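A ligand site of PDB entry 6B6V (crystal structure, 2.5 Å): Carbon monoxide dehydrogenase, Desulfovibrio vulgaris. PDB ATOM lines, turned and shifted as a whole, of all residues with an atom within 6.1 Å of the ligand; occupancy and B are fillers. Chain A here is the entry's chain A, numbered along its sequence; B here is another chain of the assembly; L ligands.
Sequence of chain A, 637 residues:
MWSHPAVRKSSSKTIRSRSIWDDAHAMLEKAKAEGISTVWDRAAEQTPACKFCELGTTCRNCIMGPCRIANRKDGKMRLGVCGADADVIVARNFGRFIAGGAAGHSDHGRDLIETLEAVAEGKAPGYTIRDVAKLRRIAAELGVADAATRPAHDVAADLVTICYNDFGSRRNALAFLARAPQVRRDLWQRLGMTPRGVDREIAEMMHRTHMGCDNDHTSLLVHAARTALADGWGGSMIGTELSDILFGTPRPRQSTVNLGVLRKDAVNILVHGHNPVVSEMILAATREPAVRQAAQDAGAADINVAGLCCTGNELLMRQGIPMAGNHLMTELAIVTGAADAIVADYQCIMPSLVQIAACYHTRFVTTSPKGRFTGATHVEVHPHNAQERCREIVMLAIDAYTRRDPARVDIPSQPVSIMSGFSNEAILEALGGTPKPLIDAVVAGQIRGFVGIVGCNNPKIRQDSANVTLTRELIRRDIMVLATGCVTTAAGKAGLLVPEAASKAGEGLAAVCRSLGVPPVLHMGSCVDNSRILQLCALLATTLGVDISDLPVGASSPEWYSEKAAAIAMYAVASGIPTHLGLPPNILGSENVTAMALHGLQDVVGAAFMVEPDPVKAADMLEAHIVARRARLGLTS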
ATOM      1  N   GLY A 273      21.846  10.868 -19.535  1.00  0.00           N
ATOM      2  CA  GLY A 273      22.328  11.250 -20.852  1.00  0.00           C
ATOM      3  C   GLY A 273      21.463  10.661 -21.960  1.00  0.00           C
ATOM      4  O   GLY A 273      20.236  10.577 -21.835  1.00  0.00           O
ATOM      5  N   HIS A 274      22.118  10.258 -23.048  1.00  0.00           N
ATOM      6  CA  HIS A 274      21.371   9.892 -24.251  1.00  0.00           C
ATOM      7  C   HIS A 274      21.844   8.606 -24.918  1.00  0.00           C
ATOM      8  O   HIS A 274      21.007   7.818 -25.365  1.00  0.00           O
ATOM      9  CB  HIS A 274      21.424  11.049 -25.254  1.00  0.00           C
ATOM     10  CG  HIS A 274      20.499  12.178 -24.918  1.00  0.00           C
ATOM     11  ND1 HIS A 274      20.728  13.048 -23.868  1.00  0.00           N
ATOM     12  CD2 HIS A 274      19.329  12.562 -25.476  1.00  0.00           C
ATOM     13  CE1 HIS A 274      19.739  13.932 -23.805  1.00  0.00           C
ATOM     14  NE2 HIS A 274      18.878  13.649 -24.766  1.00  0.00           N
ATOM     15  N   CYS A 309      16.166  10.443 -18.144  1.00  0.00           N
ATOM     16  CA  CYS A 309      16.081  11.120 -19.450  1.00  0.00           C
ATOM     17  C   CYS A 309      16.162  10.060 -20.553  1.00  0.00           C
ATOM     18  O   CYS A 309      15.592   8.969 -20.407  1.00  0.00           O
ATOM     19  CB  CYS A 309      17.137  12.204 -19.514  1.00  0.00           C
ATOM     20  SG  CYS A 309      16.770  13.599 -18.429  1.00  0.00           S
ATOM     21  N   CYS A 310      16.848  10.349 -21.673  1.00  0.00           N
ATOM     22  CA  CYS A 310      16.705   9.514 -22.858  1.00  0.00           C
ATOM     23  C   CYS A 310      17.465   8.201 -22.745  1.00  0.00           C
ATOM     24  O   CYS A 310      16.988   7.161 -23.226  1.00  0.00           O
ATOM     25  CB  CYS A 310      17.145  10.277 -24.108  1.00  0.00           C
ATOM     26  SG  CYS A 310      15.875  11.378 -24.751  1.00  0.00           S
ATOM     27  N   ASN A 326      12.464  12.282 -15.239  1.00  0.00           N
ATOM     28  CA  ASN A 326      12.800  13.045 -16.420  1.00  0.00           C
ATOM     29  C   ASN A 326      13.642  14.257 -16.026  1.00  0.00           C
ATOM     30  O   ASN A 326      14.232  14.298 -14.936  1.00  0.00           O
ATOM     31  CB  ASN A 326      11.514  13.411 -17.169  1.00  0.00           C
ATOM     32  CG  ASN A 326      10.460  14.014 -16.261  1.00  0.00           C
ATOM     33  OD1 ASN A 326      10.735  14.372 -15.118  1.00  0.00           O
ATOM     34  ND2 ASN A 326       9.241  14.120 -16.779  1.00  0.00           N
ATOM     35  N   HIS A 327      13.660  15.267 -16.901  1.00  0.00           N
ATOM     36  CA  HIS A 327      14.625  16.360 -16.825  1.00  0.00           C
ATOM     37  C   HIS A 327      14.674  17.011 -15.445  1.00  0.00           C
ATOM     38  O   HIS A 327      15.689  16.966 -14.750  1.00  0.00           O
ATOM     39  CB  HIS A 327      14.319  17.387 -17.912  1.00  0.00           C
ATOM     40  CG  HIS A 327      15.134  18.632 -17.825  1.00  0.00           C
ATOM     41  ND1 HIS A 327      16.484  18.616 -17.557  1.00  0.00           N
ATOM     42  CD2 HIS A 327      14.799  19.939 -17.973  1.00  0.00           C
ATOM     43  CE1 HIS A 327      16.949  19.862 -17.539  1.00  0.00           C
ATOM     44  NE2 HIS A 327      15.940  20.672 -17.789  1.00  0.00           N
ATOM     45  N   GLN A 347      24.610  15.469 -23.141  1.00  0.00           N
ATOM     46  CA  GLN A 347      23.373  16.191 -23.435  1.00  0.00           C
ATOM     47  C   GLN A 347      22.405  16.187 -22.259  1.00  0.00           C
ATOM     48  O   GLN A 347      22.062  15.123 -21.719  1.00  0.00           O
ATOM     49  CB  GLN A 347      22.679  15.621 -24.670  1.00  0.00           C
ATOM     50  CG  GLN A 347      23.511  15.662 -25.939  1.00  0.00           C
ATOM     51  CD  GLN A 347      22.869  14.897 -27.074  1.00  0.00           C
ATOM     52  OE1 GLN A 347      21.682  14.587 -27.025  1.00  0.00           O
ATOM     53  NE2 GLN A 347      23.654  14.569 -28.088  1.00  0.00           N
ATOM     54  N   CYS A 348      21.967  17.379 -21.853  1.00  0.00           N
ATOM     55  CA  CYS A 348      20.937  17.594 -20.836  1.00  0.00           C
ATOM     56  C   CYS A 348      21.382  17.208 -19.433  1.00  0.00           C
ATOM     57  O   CYS A 348      20.548  17.041 -18.543  1.00  0.00           O
ATOM     58  CB  CYS A 348      19.638  16.855 -21.187  1.00  0.00           C
ATOM     59  SG  CYS A 348      18.891  17.359 -22.735  1.00  0.00           S
ATOM     60  N   VAL A 454       6.098  15.113 -27.436  1.00  0.00           N
ATOM     61  CA  VAL A 454       7.527  14.926 -27.292  1.00  0.00           C
ATOM     62  C   VAL A 454       8.085  16.099 -26.492  1.00  0.00           C
ATOM     63  O   VAL A 454       7.401  17.079 -26.231  1.00  0.00           O
ATOM     64  CB  VAL A 454       8.236  14.839 -28.671  1.00  0.00           C
ATOM     65  CG1 VAL A 454       7.503  13.852 -29.563  1.00  0.00           C
ATOM     66  CG2 VAL A 454       8.274  16.195 -29.338  1.00  0.00           C
ATOM     67  N   GLY A 455       9.333  15.972 -26.069  1.00  0.00           N
ATOM     68  CA  GLY A 455      10.046  17.109 -25.510  1.00  0.00           C
ATOM     69  C   GLY A 455      10.229  17.043 -23.998  1.00  0.00           C
ATOM     70  O   GLY A 455      10.038  16.008 -23.357  1.00  0.00           O
ATOM     71  N   CYS A 456      10.583  18.202 -23.439  1.00  0.00           N
ATOM     72  CA  CYS A 456      11.283  18.298 -22.174  1.00  0.00           C
ATOM     73  C   CYS A 456      10.369  18.738 -21.037  1.00  0.00           C
ATOM     74  O   CYS A 456       9.147  18.740 -21.144  1.00  0.00           O
ATOM     75  CB  CYS A 456      12.460  19.276 -22.310  1.00  0.00           C
ATOM     76  SG  CYS A 456      13.276  19.313 -23.936  1.00  0.00           S
ATOM     77  N   ASN A 457      10.995  19.104 -19.908  1.00  0.00           N
ATOM     78  CA  ASN A 457      10.444  19.972 -18.879  1.00  0.00           C
ATOM     79  C   ASN A 457      11.114  21.342 -18.977  1.00  0.00           C
ATOM     80  O   ASN A 457      12.179  21.502 -19.585  1.00  0.00           O
ATOM     81  CB  ASN A 457      10.668  19.408 -17.474  1.00  0.00           C
ATOM     82  CG  ASN A 457       9.839  18.184 -17.186  1.00  0.00           C
ATOM     83  OD1 ASN A 457       8.734  18.013 -17.719  1.00  0.00           O
ATOM     84  ND2 ASN A 457      10.353  17.311 -16.327  1.00  0.00           N
ATOM     85  N   THR A 484       7.436  10.299 -26.488  1.00  0.00           N
ATOM     86  CA  THR A 484       8.873  10.075 -26.464  1.00  0.00           C
ATOM     87  C   THR A 484       9.502  11.057 -25.477  1.00  0.00           C
ATOM     88  O   THR A 484       8.827  11.921 -24.910  1.00  0.00           O
ATOM     89  CB  THR A 484       9.504  10.241 -27.860  1.00  0.00           C
ATOM     90  OG1 THR A 484       9.280  11.574 -28.334  1.00  0.00           O
ATOM     91  CG2 THR A 484       8.939   9.232 -28.845  1.00  0.00           C
ATOM     92  N   GLY A 485      10.807  10.900 -25.270  1.00  0.00           N
ATOM     93  CA  GLY A 485      11.560  11.812 -24.446  1.00  0.00           C
ATOM     94  C   GLY A 485      11.028  11.887 -23.022  1.00  0.00           C
ATOM     95  O   GLY A 485      10.510  10.908 -22.460  1.00  0.00           O
ATOM     96  N   CYS A 486      11.153  13.075 -22.433  1.00  0.00           N
ATOM     97  CA  CYS A 486      10.782  13.241 -21.042  1.00  0.00           C
ATOM     98  C   CYS A 486       9.277  13.251 -20.827  1.00  0.00           C
ATOM     99  O   CYS A 486       8.815  13.107 -19.685  1.00  0.00           O
ATOM    100  CB  CYS A 486      11.410  14.527 -20.502  1.00  0.00           C
ATOM    101  SG  CYS A 486      13.195  14.373 -20.252  1.00  0.00           S
ATOM    102  N   VAL A 487       8.489  13.421 -21.902  1.00  0.00           N
ATOM    103  CA  VAL A 487       7.040  13.253 -21.807  1.00  0.00           C
ATOM    104  C   VAL A 487       6.695  11.851 -21.310  1.00  0.00           C
ATOM    105  O   VAL A 487       5.691  11.661 -20.610  1.00  0.00           O
ATOM    106  CB  VAL A 487       6.398  13.542 -23.169  1.00  0.00           C
ATOM    107  CG1 VAL A 487       4.915  13.252 -23.138  1.00  0.00           C
ATOM    108  CG2 VAL A 487       6.663  14.989 -23.578  1.00  0.00           C
ATOM    109  N   SER A 526      13.105   7.328 -27.146  1.00  0.00           N
ATOM    110  CA  SER A 526      13.879   8.500 -26.767  1.00  0.00           C
ATOM    111  C   SER A 526      13.634   9.636 -27.752  1.00  0.00           C
ATOM    112  O   SER A 526      12.700   9.607 -28.558  1.00  0.00           O
ATOM    113  CB  SER A 526      15.357   8.138 -26.701  1.00  0.00           C
ATOM    114  OG  SER A 526      15.785   7.565 -27.929  1.00  0.00           O
ATOM    115  N   CYS A 527      14.495  10.646 -27.702  1.00  0.00           N
ATOM    116  CA  CYS A 527      14.358  11.787 -28.608  1.00  0.00           C
ATOM    117  C   CYS A 527      14.839  11.469 -30.016  1.00  0.00           C
ATOM    118  O   CYS A 527      14.274  11.989 -30.980  1.00  0.00           O
ATOM    119  CB  CYS A 527      15.106  12.989 -28.035  1.00  0.00           C
ATOM    120  SG  CYS A 527      14.204  13.677 -26.636  1.00  0.00           S
ATOM    121  N   TYR A 561      12.612  22.708 -23.736  1.00  0.00           N
ATOM    122  CA  TYR A 561      13.652  23.681 -23.381  1.00  0.00           C
ATOM    123  C   TYR A 561      14.841  23.703 -24.332  1.00  0.00           C
ATOM    124  O   TYR A 561      15.406  24.775 -24.543  1.00  0.00           O
ATOM    125  CB  TYR A 561      14.166  23.415 -21.944  1.00  0.00           C
ATOM    126  CG  TYR A 561      15.430  22.577 -21.919  1.00  0.00           C
ATOM    127  CD1 TYR A 561      16.691  23.172 -21.910  1.00  0.00           C
ATOM    128  CD2 TYR A 561      15.361  21.201 -21.941  1.00  0.00           C
ATOM    129  CE1 TYR A 561      17.848  22.405 -21.919  1.00  0.00           C
ATOM    130  CE2 TYR A 561      16.505  20.427 -21.942  1.00  0.00           C
ATOM    131  CZ  TYR A 561      17.740  21.037 -21.926  1.00  0.00           C
ATOM    132  OH  TYR A 561      18.874  20.254 -21.929  1.00  0.00           O
ATOM    133  N   SER A 562      15.235  22.573 -24.927  1.00  0.00           N
ATOM    134  CA  SER A 562      16.552  22.423 -25.514  1.00  0.00           C
ATOM    135  C   SER A 562      16.586  22.782 -27.002  1.00  0.00           C
ATOM    136  O   SER A 562      15.555  22.911 -27.664  1.00  0.00           O
ATOM    137  CB  SER A 562      17.057  20.999 -25.323  1.00  0.00           C
ATOM    138  OG  SER A 562      16.216  20.075 -26.009  1.00  0.00           O
ATOM    139  N   LYS A 564      17.687  20.699 -29.156  1.00  0.00           N
ATOM    140  CA  LYS A 564      17.239  19.496 -29.854  1.00  0.00           C
ATOM    141  C   LYS A 564      15.729  19.474 -30.017  1.00  0.00           C
ATOM    142  O   LYS A 564      15.223  19.060 -31.068  1.00  0.00           O
ATOM    143  CB  LYS A 564      17.730  18.261 -29.118  1.00  0.00           C
ATOM    144  CG  LYS A 564      19.229  18.029 -29.271  1.00  0.00           C
ATOM    145  CD  LYS A 564      19.689  16.838 -28.438  1.00  0.00           C
ATOM    146  CE  LYS A 564      19.463  17.092 -26.958  1.00  0.00           C
ATOM    147  NZ  LYS A 564      19.727  15.880 -26.144  1.00  0.00           N
ATOM    148  N   ALA A 565      14.989  19.918 -28.991  1.00  0.00           N
ATOM    149  CA  ALA A 565      13.535  19.987 -29.117  1.00  0.00           C
ATOM    150  C   ALA A 565      13.116  20.946 -30.216  1.00  0.00           C
ATOM    151  O   ALA A 565      12.146  20.694 -30.938  1.00  0.00           O
ATOM    152  CB  ALA A 565      12.916  20.391 -27.775  1.00  0.00           C
ATOM    153  N   ILE A 568      13.783  19.072 -33.492  1.00  0.00           N
ATOM    154  CA  ILE A 568      12.766  18.056 -33.742  1.00  0.00           C
ATOM    155  C   ILE A 568      11.489  18.717 -34.248  1.00  0.00           C
ATOM    156  O   ILE A 568      10.862  18.257 -35.208  1.00  0.00           O
ATOM    157  CB  ILE A 568      12.501  17.233 -32.466  1.00  0.00           C
ATOM    158  CG1 ILE A 568      13.737  16.396 -32.133  1.00  0.00           C
ATOM    159  CG2 ILE A 568      11.286  16.342 -32.638  1.00  0.00           C
ATOM    160  CD1 ILE A 568      13.693  15.774 -30.753  1.00  0.00           C
ATOM    161  N   HIS B 210      26.015  22.515 -26.661  1.00  0.00           N
ATOM    162  CA  HIS B 210      24.638  22.305 -26.237  1.00  0.00           C
ATOM    163  C   HIS B 210      24.577  22.145 -24.727  1.00  0.00           C
ATOM    164  O   HIS B 210      25.523  21.690 -24.091  1.00  0.00           O
ATOM    165  CB  HIS B 210      24.070  21.062 -26.926  1.00  0.00           C
ATOM    166  CG  HIS B 210      22.617  20.812 -26.656  1.00  0.00           C
ATOM    167  ND1 HIS B 210      22.149  20.364 -25.447  1.00  0.00           N
ATOM    168  CD2 HIS B 210      21.527  20.923 -27.463  1.00  0.00           C
ATOM    169  CE1 HIS B 210      20.835  20.232 -25.501  1.00  0.00           C
ATOM    170  NE2 HIS B 210      20.434  20.556 -26.716  1.00  0.00           N
HETATM  171 FE1  LIG L   1      16.783  16.523 -22.951  1.00  0.00          FE
HETATM  172 FE2  LIG L   1      16.602  13.526 -24.557  1.00  0.00          FE
HETATM  173 FE3  LIG L   1      14.446  17.375 -23.686  1.00  0.00          FE
HETATM  174 FE4  LIG L   1      14.371  15.268 -21.989  1.00  0.00          FE
HETATM  175  S1  LIG L   1      13.102  15.448 -23.817  1.00  0.00           S
HETATM  176  S2  LIG L   1      15.174  17.352 -21.502  1.00  0.00           S
HETATM  177  S3  LIG L   1      16.151  17.101 -25.183  1.00  0.00           S
HETATM  178  S4  LIG L   1      16.392  14.335 -22.430  1.00  0.00           S
HETATM  179 NI1  LIG L   1      14.792  15.243 -25.231  1.00  0.00          NI
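S1 of the ligand lies close to N of Cys 486 (3.4 Å).
An iron atom (FE1) of the ligand is bound by the side-chain sulfur (SG) of Cys 348 (2.3 Å).
A ring nitrogen (NE2) of His 274 is bound to an iron atom (FE2) of the ligand (2.3 Å).
FE3 of the ligand is bound by SG of Cys 456.
The side-chain hydroxyl (OG) of Ser 562 lies close to a sulfur (S3) of the ligand.
A nickel atom (NI1) of the ligand is bound by the side-chain sulfur (SG) of Cys 527 (2.2 Å).
N of Cys 456 lies close to S1 of the ligand.
An iron atom (FE2) of the ligand is bound by the side-chain sulfur (SG) of Cys 310, at 2.3 Å.
The side-chain sulfur of Cys 486 binds an iron atom (FE4) of the ligand (2.3 Å).
A ring nitrogen (NE2) of His 274 lies close to the side-chain amino group (NZ) of Lys 564, at 2.8 Å.
O of Gly 455 sits at hydrogen-bond distance from N of Val 487 (3.3 Å).
N of His 327 sits close to SG of Cys 486.
The backbone NH (N) of Tyr 561 sits close to the side-chain sulfur (SG) of Cys 456 (3.5 Å).
NZ of Lys 564 is in hydrogen-bond range of OE1 of Gln 347 (2.5 Å).
The backbone NH (N) of Cys 486 sits at hydrogen-bond distance from the backbone carbonyl oxygen (O) of Gly 455.
The side-chain sulfur (SG) of Cys 348 lies close to the side-chain hydroxyl (OH) of Tyr 561, at 3.0 Å.
O of Gly 273 sits at hydrogen-bond distance from N of Cys 310 (3.4 Å).
The backbone carbonyl oxygen (O) of Gly 455 sits close to a sulfur (S1) of the ligand (3.1 Å).
Residues that only touch the ligand: Tyr 561, Cys 309, His 327, Lys 564 and Gly 485.
Within 4 Å of the ligand: His 274, Cys 309, Cys 310, His 327, Cys 348, Gly 455, Cys 456, Gly 485, Cys 486, Cys 527, Tyr 561, Ser 562 and Lys 564.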
